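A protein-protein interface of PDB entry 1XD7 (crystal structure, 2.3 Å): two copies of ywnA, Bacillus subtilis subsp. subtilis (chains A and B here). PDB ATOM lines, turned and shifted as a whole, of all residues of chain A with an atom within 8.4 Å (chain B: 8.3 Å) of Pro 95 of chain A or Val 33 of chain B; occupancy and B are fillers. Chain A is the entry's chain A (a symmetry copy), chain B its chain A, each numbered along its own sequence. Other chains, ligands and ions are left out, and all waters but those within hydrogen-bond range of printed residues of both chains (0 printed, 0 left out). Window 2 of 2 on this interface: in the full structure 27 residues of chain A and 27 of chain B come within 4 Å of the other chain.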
ATOM      1  N   ASN A  94      27.337  21.783   3.984  1.00  0.00           N
ATOM      2  CA  ASN A  94      26.234  22.455   4.653  1.00  0.00           C
ATOM      3  C   ASN A  94      24.840  22.083   4.148  1.00  0.00           C
ATOM      4  O   ASN A  94      23.871  22.755   4.502  1.00  0.00           O
ATOM      5  CB  ASN A  94      26.408  23.978   4.564  1.00  0.00           C
ATOM      6  CG  ASN A  94      27.484  24.503   5.504  1.00  0.00           C
ATOM      7  OD1 ASN A  94      27.880  25.669   5.427  1.00  0.00           O
ATOM      8  ND2 ASN A  94      27.955  23.644   6.403  1.00  0.00           N
ATOM      9  N   PRO A  95      24.704  21.023   3.319  1.00  0.00           N
ATOM     10  CA  PRO A  95      25.659  20.067   2.738  1.00  0.00           C
ATOM     11  C   PRO A  95      26.038  20.384   1.279  1.00  0.00           C
ATOM     12  O   PRO A  95      25.415  21.224   0.630  1.00  0.00           O
ATOM     13  CB  PRO A  95      24.915  18.747   2.861  1.00  0.00           C
ATOM     14  CG  PRO A  95      23.534  19.158   2.488  1.00  0.00           C
ATOM     15  CD  PRO A  95      23.335  20.476   3.233  1.00  0.00           C
ATOM     16  N   LYS A  96      27.053  19.699   0.766  1.00  0.00           N
ATOM     17  CA  LYS A  96      27.510  19.932  -0.601  1.00  0.00           C
ATOM     18  C   LYS A  96      26.965  18.913  -1.582  1.00  0.00           C
ATOM     19  O   LYS A  96      26.521  19.274  -2.663  1.00  0.00           O
ATOM     20  CB  LYS A  96      29.039  19.934  -0.642  1.00  0.00           C
ATOM     21  CG  LYS A  96      29.665  21.129   0.077  1.00  0.00           C
ATOM     22  CD  LYS A  96      31.174  20.972   0.276  1.00  0.00           C
ATOM     23  CE  LYS A  96      31.506  19.791   1.194  1.00  0.00           C
ATOM     24  NZ  LYS A  96      32.971  19.680   1.484  1.00  0.00           N
ATOM     25  N   CYS A  97      26.999  17.641  -1.206  1.00  0.00           N
ATOM     26  CA  CYS A  97      26.494  16.588  -2.073  1.00  0.00           C
ATOM     27  C   CYS A  97      25.089  16.938  -2.562  1.00  0.00           C
ATOM     28  O   CYS A  97      24.335  17.612  -1.866  1.00  0.00           O
ATOM     29  CB  CYS A  97      26.460  15.256  -1.323  1.00  0.00           C
ATOM     30  SG  CYS A  97      26.031  13.861  -2.387  1.00  0.00           S
ATOM     31  N   PRO A  98      24.720  16.493  -3.777  1.00  0.00           N
ATOM     32  CA  PRO A  98      23.387  16.792  -4.307  1.00  0.00           C
ATOM     33  C   PRO A  98      22.329  16.065  -3.492  1.00  0.00           C
ATOM     34  O   PRO A  98      21.216  16.557  -3.312  1.00  0.00           O
ATOM     35  CB  PRO A  98      23.452  16.261  -5.736  1.00  0.00           C
ATOM     36  CG  PRO A  98      24.899  16.327  -6.065  1.00  0.00           C
ATOM     37  CD  PRO A  98      25.537  15.827  -4.803  1.00  0.00           C
ATOM     38  N   VAL A  99      22.695  14.884  -3.008  1.00  0.00           N
ATOM     39  CA  VAL A  99      21.792  14.079  -2.213  1.00  0.00           C
ATOM     40  C   VAL A  99      21.466  14.825  -0.934  1.00  0.00           C
ATOM     41  O   VAL A  99      20.303  14.940  -0.545  1.00  0.00           O
ATOM     42  CB  VAL A  99      22.424  12.759  -1.842  1.00  0.00           C
ATOM     43  CG1 VAL A  99      21.347  11.752  -1.535  1.00  0.00           C
ATOM     44  CG2 VAL A  99      23.307  12.277  -2.975  1.00  0.00           C
ATOM     45  N   GLY A 100      22.506  15.337  -0.286  1.00  0.00           N
ATOM     46  CA  GLY A 100      22.314  16.076   0.942  1.00  0.00           C
ATOM     47  C   GLY A 100      21.332  17.206   0.734  1.00  0.00           C
ATOM     48  O   GLY A 100      20.377  17.353   1.487  1.00  0.00           O
ATOM     49  N   LYS A 101      21.563  18.008  -0.293  1.00  0.00           N
ATOM     50  CA  LYS A 101      20.679  19.118  -0.570  1.00  0.00           C
ATOM     51  C   LYS A 101      19.254  18.644  -0.738  1.00  0.00           C
ATOM     52  O   LYS A 101      18.325  19.248  -0.194  1.00  0.00           O
ATOM     53  CB  LYS A 101      21.102  19.855  -1.837  1.00  0.00           C
ATOM     54  CG  LYS A 101      22.324  20.741  -1.699  1.00  0.00           C
ATOM     55  CD  LYS A 101      22.534  21.515  -3.003  1.00  0.00           C
ATOM     56  CE  LYS A 101      23.518  22.660  -2.868  1.00  0.00           C
ATOM     57  NZ  LYS A 101      23.176  23.745  -3.860  1.00  0.00           N
ATOM     58  N   LYS A 102      19.068  17.574  -1.502  1.00  0.00           N
ATOM     59  CA  LYS A 102      17.721  17.059  -1.723  1.00  0.00           C
ATOM     60  C   LYS A 102      17.043  16.905  -0.377  1.00  0.00           C
ATOM     61  O   LYS A 102      16.043  17.561  -0.088  1.00  0.00           O
ATOM     62  CB  LYS A 102      17.752  15.698  -2.429  1.00  0.00           C
ATOM     63  CG  LYS A 102      17.881  15.750  -3.950  1.00  0.00           C
ATOM     64  CD  LYS A 102      16.698  16.447  -4.593  1.00  0.00           C
ATOM     65  CE  LYS A 102      16.784  16.401  -6.117  1.00  0.00           C
ATOM     66  NZ  LYS A 102      15.896  17.419  -6.755  1.00  0.00           N
ATOM     67  N   ILE A 103      17.615  16.027   0.438  1.00  0.00           N
ATOM     68  CA  ILE A 103      17.112  15.751   1.767  1.00  0.00           C
ATOM     69  C   ILE A 103      16.860  17.068   2.485  1.00  0.00           C
ATOM     70  O   ILE A 103      15.843  17.238   3.159  1.00  0.00           O
ATOM     71  CB  ILE A 103      18.128  14.912   2.565  1.00  0.00           C
ATOM     72  CG1 ILE A 103      18.251  13.526   1.938  1.00  0.00           C
ATOM     73  CG2 ILE A 103      17.689  14.794   4.017  1.00  0.00           C
ATOM     74  CD1 ILE A 103      19.335  12.661   2.537  1.00  0.00           C
ATOM     75  N   GLN A 104      17.782  18.006   2.318  1.00  0.00           N
ATOM     76  CA  GLN A 104      17.634  19.292   2.963  1.00  0.00           C
ATOM     77  C   GLN A 104      16.250  19.812   2.662  1.00  0.00           C
ATOM     78  O   GLN A 104      15.499  20.162   3.564  1.00  0.00           O
ATOM     79  CB  GLN A 104      18.675  20.284   2.455  1.00  0.00           C
ATOM     80  CG  GLN A 104      18.525  21.658   3.069  1.00  0.00           C
ATOM     81  CD  GLN A 104      18.622  21.634   4.593  1.00  0.00           C
ATOM     82  OE1 GLN A 104      18.286  22.619   5.261  1.00  0.00           O
ATOM     83  NE2 GLN A 104      19.088  20.514   5.150  1.00  0.00           N
ATOM     84  N   ASN A 105      15.912  19.847   1.383  1.00  0.00           N
ATOM     85  CA  ASN A 105      14.607  20.327   0.984  1.00  0.00           C
ATOM     86  C   ASN A 105      13.493  19.568   1.661  1.00  0.00           C
ATOM     87  O   ASN A 105      12.516  20.168   2.088  1.00  0.00           O
ATOM     88  CB  ASN A 105      14.444  20.237  -0.525  1.00  0.00           C
ATOM     89  CG  ASN A 105      15.291  21.246  -1.242  1.00  0.00           C
ATOM     90  OD1 ASN A 105      15.347  22.406  -0.841  1.00  0.00           O
ATOM     91  ND2 ASN A 105      15.954  20.822  -2.312  1.00  0.00           N
ATOM     92  N   ASP A 108      13.469  20.879   5.080  1.00  0.00           N
ATOM     93  CA  ASP A 108      12.984  22.251   5.058  1.00  0.00           C
ATOM     94  C   ASP A 108      11.470  22.366   5.140  1.00  0.00           C
ATOM     95  O   ASP A 108      10.930  23.127   5.946  1.00  0.00           O
ATOM     96  CB  ASP A 108      13.464  22.959   3.789  1.00  0.00           C
ATOM     97  CG  ASP A 108      14.797  23.654   3.974  1.00  0.00           C
ATOM     98  OD1 ASP A 108      15.602  23.167   4.784  1.00  0.00           O
ATOM     99  OD2 ASP A 108      15.042  24.679   3.300  1.00  0.00           O
ATOM    100  N   ALA B   9      17.726  17.554  12.284  1.00  0.00           N
ATOM    101  CA  ALA B   9      18.100  17.592  10.889  1.00  0.00           C
ATOM    102  C   ALA B   9      19.355  16.742  10.699  1.00  0.00           C
ATOM    103  O   ALA B   9      19.378  15.803   9.893  1.00  0.00           O
ATOM    104  CB  ALA B   9      18.362  19.023  10.466  1.00  0.00           C
ATOM    105  N   VAL B  10      20.402  17.054  11.455  1.00  0.00           N
ATOM    106  CA  VAL B  10      21.637  16.291  11.319  1.00  0.00           C
ATOM    107  C   VAL B  10      21.371  14.810  11.558  1.00  0.00           C
ATOM    108  O   VAL B  10      21.954  13.946  10.886  1.00  0.00           O
ATOM    109  CB  VAL B  10      22.736  16.828  12.286  1.00  0.00           C
ATOM    110  CG1 VAL B  10      23.874  15.851  12.406  1.00  0.00           C
ATOM    111  CG2 VAL B  10      23.264  18.165  11.758  1.00  0.00           C
ATOM    112  N   ALA B  11      20.484  14.503  12.496  1.00  0.00           N
ATOM    113  CA  ALA B  11      20.194  13.101  12.749  1.00  0.00           C
ATOM    114  C   ALA B  11      19.487  12.491  11.536  1.00  0.00           C
ATOM    115  O   ALA B  11      19.682  11.322  11.229  1.00  0.00           O
ATOM    116  CB  ALA B  11      19.345  12.946  13.999  1.00  0.00           C
ATOM    117  N   ILE B  12      18.679  13.290  10.845  1.00  0.00           N
ATOM    118  CA  ILE B  12      17.958  12.814   9.665  1.00  0.00           C
ATOM    119  C   ILE B  12      18.900  12.536   8.475  1.00  0.00           C
ATOM    120  O   ILE B  12      18.809  11.477   7.837  1.00  0.00           O
ATOM    121  CB  ILE B  12      16.875  13.824   9.229  1.00  0.00           C
ATOM    122  CG1 ILE B  12      15.913  14.100  10.389  1.00  0.00           C
ATOM    123  CG2 ILE B  12      16.090  13.265   8.065  1.00  0.00           C
ATOM    124  CD1 ILE B  12      15.111  12.891  10.820  1.00  0.00           C
ATOM    125  N   HIS B  13      19.796  13.470   8.170  1.00  0.00           N
ATOM    126  CA  HIS B  13      20.749  13.250   7.077  1.00  0.00           C
ATOM    127  C   HIS B  13      21.488  11.959   7.331  1.00  0.00           C
ATOM    128  O   HIS B  13      21.627  11.109   6.449  1.00  0.00           O
ATOM    129  CB  HIS B  13      21.773  14.377   7.014  1.00  0.00           C
ATOM    130  CG  HIS B  13      21.275  15.587   6.310  1.00  0.00           C
ATOM    131  ND1 HIS B  13      21.135  15.640   4.942  1.00  0.00           N
ATOM    132  CD2 HIS B  13      20.815  16.770   6.779  1.00  0.00           C
ATOM    133  CE1 HIS B  13      20.611  16.804   4.597  1.00  0.00           C
ATOM    134  NE2 HIS B  13      20.405  17.509   5.696  1.00  0.00           N
ATOM    135  N   ILE B  14      21.959  11.818   8.560  1.00  0.00           N
ATOM    136  CA  ILE B  14      22.709  10.641   8.944  1.00  0.00           C
ATOM    137  C   ILE B  14      21.892   9.393   8.675  1.00  0.00           C
ATOM    138  O   ILE B  14      22.364   8.458   8.021  1.00  0.00           O
ATOM    139  CB  ILE B  14      23.084  10.718  10.429  1.00  0.00           C
ATOM    140  CG1 ILE B  14      24.087  11.853  10.633  1.00  0.00           C
ATOM    141  CG2 ILE B  14      23.649   9.417  10.901  1.00  0.00           C
ATOM    142  CD1 ILE B  14      24.429  12.131  12.092  1.00  0.00           C
ATOM    143  N   LEU B  15      20.664   9.371   9.178  1.00  0.00           N
ATOM    144  CA  LEU B  15      19.821   8.207   8.980  1.00  0.00           C
ATOM    145  C   LEU B  15      19.531   7.951   7.514  1.00  0.00           C
ATOM    146  O   LEU B  15      19.508   6.811   7.087  1.00  0.00           O
ATOM    147  CB  LEU B  15      18.518   8.369   9.748  1.00  0.00           C
ATOM    148  CG  LEU B  15      18.742   8.310  11.258  1.00  0.00           C
ATOM    149  CD1 LEU B  15      17.450   8.642  11.985  1.00  0.00           C
ATOM    150  CD2 LEU B  15      19.241   6.931  11.646  1.00  0.00           C
ATOM    151  N   SER B  16      19.300   9.010   6.746  1.00  0.00           N
ATOM    152  CA  SER B  16      19.028   8.850   5.321  1.00  0.00           C
ATOM    153  C   SER B  16      20.128   8.054   4.635  1.00  0.00           C
ATOM    154  O   SER B  16      19.874   7.037   4.009  1.00  0.00           O
ATOM    155  CB  SER B  16      18.905  10.210   4.650  1.00  0.00           C
ATOM    156  OG  SER B  16      17.758  10.883   5.131  1.00  0.00           O
ATOM    157  N   LEU B  17      21.361   8.520   4.767  1.00  0.00           N
ATOM    158  CA  LEU B  17      22.484   7.836   4.148  1.00  0.00           C
ATOM    159  C   LEU B  17      22.611   6.424   4.673  1.00  0.00           C
ATOM    160  O   LEU B  17      22.938   5.501   3.917  1.00  0.00           O
ATOM    161  CB  LEU B  17      23.780   8.593   4.414  1.00  0.00           C
ATOM    162  CG  LEU B  17      23.716  10.073   4.052  1.00  0.00           C
ATOM    163  CD1 LEU B  17      25.029  10.741   4.414  1.00  0.00           C
ATOM    164  CD2 LEU B  17      23.416  10.219   2.578  1.00  0.00           C
ATOM    165  N   ILE B  18      22.367   6.244   5.966  1.00  0.00           N
ATOM    166  CA  ILE B  18      22.478   4.908   6.519  1.00  0.00           C
ATOM    167  C   ILE B  18      21.411   4.064   5.878  1.00  0.00           C
ATOM    168  O   ILE B  18      21.572   2.856   5.759  1.00  0.00           O
ATOM    169  CB  ILE B  18      22.319   4.888   8.048  1.00  0.00           C
ATOM    170  CG1 ILE B  18      23.550   5.524   8.687  1.00  0.00           C
ATOM    171  CG2 ILE B  18      22.202   3.455   8.560  1.00  0.00           C
ATOM    172  CD1 ILE B  18      23.642   5.348  10.202  1.00  0.00           C
ATOM    173  N   SER B  26      31.616   6.434   9.744  1.00  0.00           N
ATOM    174  CA  SER B  26      31.121   7.670  10.308  1.00  0.00           C
ATOM    175  C   SER B  26      31.807   8.840   9.650  1.00  0.00           C
ATOM    176  O   SER B  26      31.191   9.873   9.401  1.00  0.00           O
ATOM    177  CB  SER B  26      31.376   7.688  11.811  1.00  0.00           C
ATOM    178  OG  SER B  26      30.993   6.452  12.374  1.00  0.00           O
ATOM    179  N   GLU B  27      33.093   8.672   9.367  1.00  0.00           N
ATOM    180  CA  GLU B  27      33.866   9.733   8.736  1.00  0.00           C
ATOM    181  C   GLU B  27      33.207  10.149   7.430  1.00  0.00           C
ATOM    182  O   GLU B  27      32.862  11.318   7.236  1.00  0.00           O
ATOM    183  CB  GLU B  27      35.300   9.260   8.469  1.00  0.00           C
ATOM    184  CG  GLU B  27      35.591   7.813   8.894  1.00  0.00           C
ATOM    185  CD  GLU B  27      35.956   6.890   7.716  1.00  0.00           C
ATOM    186  OE1 GLU B  27      36.308   5.702   7.959  1.00  0.00           O
ATOM    187  OE2 GLU B  27      35.883   7.353   6.553  1.00  0.00           O
ATOM    188  N   ILE B  28      33.021   9.177   6.543  1.00  0.00           N
ATOM    189  CA  ILE B  28      32.412   9.428   5.242  1.00  0.00           C
ATOM    190  C   ILE B  28      31.096  10.152   5.405  1.00  0.00           C
ATOM    191  O   ILE B  28      30.789  11.082   4.657  1.00  0.00           O
ATOM    192  CB  ILE B  28      32.168   8.113   4.487  1.00  0.00           C
ATOM    193  CG1 ILE B  28      33.487   7.351   4.370  1.00  0.00           C
ATOM    194  CG2 ILE B  28      31.617   8.399   3.094  1.00  0.00           C
ATOM    195  CD1 ILE B  28      33.356   5.978   3.780  1.00  0.00           C
ATOM    196  N   ILE B  29      30.329   9.735   6.407  1.00  0.00           N
ATOM    197  CA  ILE B  29      29.039  10.352   6.660  1.00  0.00           C
ATOM    198  C   ILE B  29      29.207  11.812   7.002  1.00  0.00           C
ATOM    199  O   ILE B  29      28.518  12.674   6.459  1.00  0.00           O
ATOM    200  CB  ILE B  29      28.319   9.608   7.774  1.00  0.00           C
ATOM    201  CG1 ILE B  29      28.119   8.156   7.327  1.00  0.00           C
ATOM    202  CG2 ILE B  29      26.997  10.288   8.096  1.00  0.00           C
ATOM    203  CD1 ILE B  29      27.395   7.275   8.296  1.00  0.00           C
ATOM    204  N   ALA B  30      30.138  12.104   7.893  1.00  0.00           N
ATOM    205  CA  ALA B  30      30.382  13.491   8.250  1.00  0.00           C
ATOM    206  C   ALA B  30      30.787  14.240   6.976  1.00  0.00           C
ATOM    207  O   ALA B  30      30.320  15.350   6.720  1.00  0.00           O
ATOM    208  CB  ALA B  30      31.484  13.575   9.306  1.00  0.00           C
ATOM    209  N   ASP B  31      31.649  13.628   6.173  1.00  0.00           N
ATOM    210  CA  ASP B  31      32.072  14.254   4.918  1.00  0.00           C
ATOM    211  C   ASP B  31      30.842  14.507   4.081  1.00  0.00           C
ATOM    212  O   ASP B  31      30.529  15.642   3.733  1.00  0.00           O
ATOM    213  CB  ASP B  31      32.987  13.335   4.120  1.00  0.00           C
ATOM    214  CG  ASP B  31      34.210  12.936   4.886  1.00  0.00           C
ATOM    215  OD1 ASP B  31      35.002  13.833   5.248  1.00  0.00           O
ATOM    216  OD2 ASP B  31      34.385  11.722   5.128  1.00  0.00           O
ATOM    217  N   SER B  32      30.152  13.421   3.757  1.00  0.00           N
ATOM    218  CA  SER B  32      28.943  13.487   2.951  1.00  0.00           C
ATOM    219  C   SER B  32      27.945  14.472   3.523  1.00  0.00           C
ATOM    220  O   SER B  32      27.314  15.227   2.788  1.00  0.00           O
ATOM    221  CB  SER B  32      28.298  12.113   2.872  1.00  0.00           C
ATOM    222  OG  SER B  32      29.258  11.137   2.515  1.00  0.00           O
ATOM    223  N   VAL B  33      27.804  14.466   4.838  1.00  0.00           N
ATOM    224  CA  VAL B  33      26.861  15.374   5.470  1.00  0.00           C
ATOM    225  C   VAL B  33      27.474  16.745   5.649  1.00  0.00           C
ATOM    226  O   VAL B  33      26.782  17.710   5.956  1.00  0.00           O
ATOM    227  CB  VAL B  33      26.420  14.849   6.848  1.00  0.00           C
ATOM    228  CG1 VAL B  33      25.520  15.844   7.512  1.00  0.00           C
ATOM    229  CG2 VAL B  33      25.702  13.535   6.685  1.00  0.00           C
ATOM    230  N   ASN B  34      28.782  16.825   5.447  1.00  0.00           N
ATOM    231  CA  ASN B  34      29.508  18.079   5.605  1.00  0.00           C
ATOM    232  C   ASN B  34      29.332  18.639   7.012  1.00  0.00           C
ATOM    233  O   ASN B  34      28.897  19.777   7.202  1.00  0.00           O
ATOM    234  CB  ASN B  34      29.049  19.117   4.579  1.00  0.00           C
ATOM    235  CG  ASN B  34      30.015  20.294   4.475  1.00  0.00           C
ATOM    236  OD1 ASN B  34      29.810  21.210   3.677  1.00  0.00           O
ATOM    237  ND2 ASN B  34      31.077  20.267   5.284  1.00  0.00           N
ATOM    238  N   THR B  35      29.679  17.813   7.991  1.00  0.00           N
ATOM    239  CA  THR B  35      29.597  18.175   9.393  1.00  0.00           C
ATOM    240  C   THR B  35      30.747  17.495  10.112  1.00  0.00           C
ATOM    241  O   THR B  35      31.355  16.554   9.595  1.00  0.00           O
ATOM    242  CB  THR B  35      28.261  17.705  10.013  1.00  0.00           C
ATOM    243  OG1 THR B  35      27.195  18.506   9.493  1.00  0.00           O
ATOM    244  CG2 THR B  35      28.284  17.832  11.529  1.00  0.00           C
ATOM    245  N   ASN B  36      31.046  17.989  11.303  1.00  0.00           N
ATOM    246  CA  ASN B  36      32.110  17.447  12.134  1.00  0.00           C
ATOM    247  C   ASN B  36      31.816  15.972  12.454  1.00  0.00           C
ATOM    248  O   ASN B  36      30.682  15.605  12.763  1.00  0.00           O
ATOM    249  CB  ASN B  36      32.186  18.305  13.410  1.00  0.00           C
ATOM    250  CG  ASN B  36      33.223  17.818  14.416  1.00  0.00           C
ATOM    251  OD1 ASN B  36      33.528  18.525  15.376  1.00  0.00           O
ATOM    252  ND2 ASN B  36      33.750  16.615  14.217  1.00  0.00           N
ATOM    253  N   VAL B  39      30.445  15.032  16.135  1.00  0.00           N
ATOM    254  CA  VAL B  39      29.016  15.270  16.184  1.00  0.00           C
ATOM    255  C   VAL B  39      28.326  14.023  15.656  1.00  0.00           C
ATOM    256  O   VAL B  39      27.463  13.434  16.318  1.00  0.00           O
ATOM    257  CB  VAL B  39      28.649  16.440  15.271  1.00  0.00           C
ATOM    258  CG1 VAL B  39      27.158  16.615  15.233  1.00  0.00           C
ATOM    259  CG2 VAL B  39      29.331  17.708  15.756  1.00  0.00           C
ATOM    260  N   VAL B  40      28.744  13.618  14.461  1.00  0.00           N
ATOM    261  CA  VAL B  40      28.195  12.452  13.801  1.00  0.00           C
ATOM    262  C   VAL B  40      28.282  11.203  14.681  1.00  0.00           C
ATOM    263  O   VAL B  40      27.289  10.489  14.880  1.00  0.00           O
ATOM    264  CB  VAL B  40      28.927  12.208  12.457  1.00  0.00           C
ATOM    265  CG1 VAL B  40      28.395  10.962  11.794  1.00  0.00           C
ATOM    266  CG2 VAL B  40      28.748  13.413  11.541  1.00  0.00           C
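The side-chain amide nitrogen (NE2) of Gln 104 of chain A lies within hydrogen-bond range of a ring nitrogen (NE2) of His 13 of chain B (3.3 Å).
N of Asn 94 of chain A sits at hydrogen-bond distance from OD1 of Asn 34 of chain B (2.6 Å).
The side-chain amide oxygen of Gln 104 of chain A lies close to the side-chain carboxylate of Asp 108 of chain A, at 2.8 Å.
The backbone carbonyl oxygen (O) of Ile 12 of chain B is in hydrogen-bond range of the side-chain hydroxyl (OG) of Ser 16 of chain B, at 3.0 Å.
CB of Pro 95 of chain A touches O of Val 33 of chain B, 3.8 Å away.
Pro 95 of chain A touches Asn 34 of chain B (CA to CB, 3.97 Å).
Asn 34 of chain B touches Lys 96 of chain A.
Gly 100 of chain A touches His 13 of chain B (O to CE1, 3.2 Å).
CG2 of Ile 103 of chain A touches CE1 of His 13 of chain B, 3.6 Å away.
CD1 of Ile 103 of chain A touches CB of Ser 16 of chain B, at 3.3 Å.
Pro 95 of chain A touches just these residues of chain B: Val 33 and Asn 34.
Val 33 of chain B touches just one residue of chain A: Pro 95 (3.8 Å).
No residue of chain A comes within 4 Å of Ser 32 of chain B.
Printed residues of chain A within 4 Å of Ser 16 of chain B: Ile 103.
Printed residues of chain A within 4 Å of His 13 of chain B: Gly 100, Ile 103 and Gln 104.
Val 99 of chain A touches none of the printed residues of chain B.
The nearest residue of chain B that does not touch Pro 95 of chain A is Ser 32 of chain B (4.3 Å).
The nearest residue of chain A that does not touch Val 33 of chain B is Asn 94 of chain A (4.6 Å).
Of the 23 printed residues of chain B, 4 touch a printed residue of chain A.
Printed residues of chain A that touch a printed residue of chain B: Asn 94, Pro 95, Lys 96, Gly 100, Ile 103 and Gln 104.
Hydrophobic or aromatic side chains of chain A that line the printed part of chain B: Pro 95 and Ile 103.
No position is printed for both chains.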
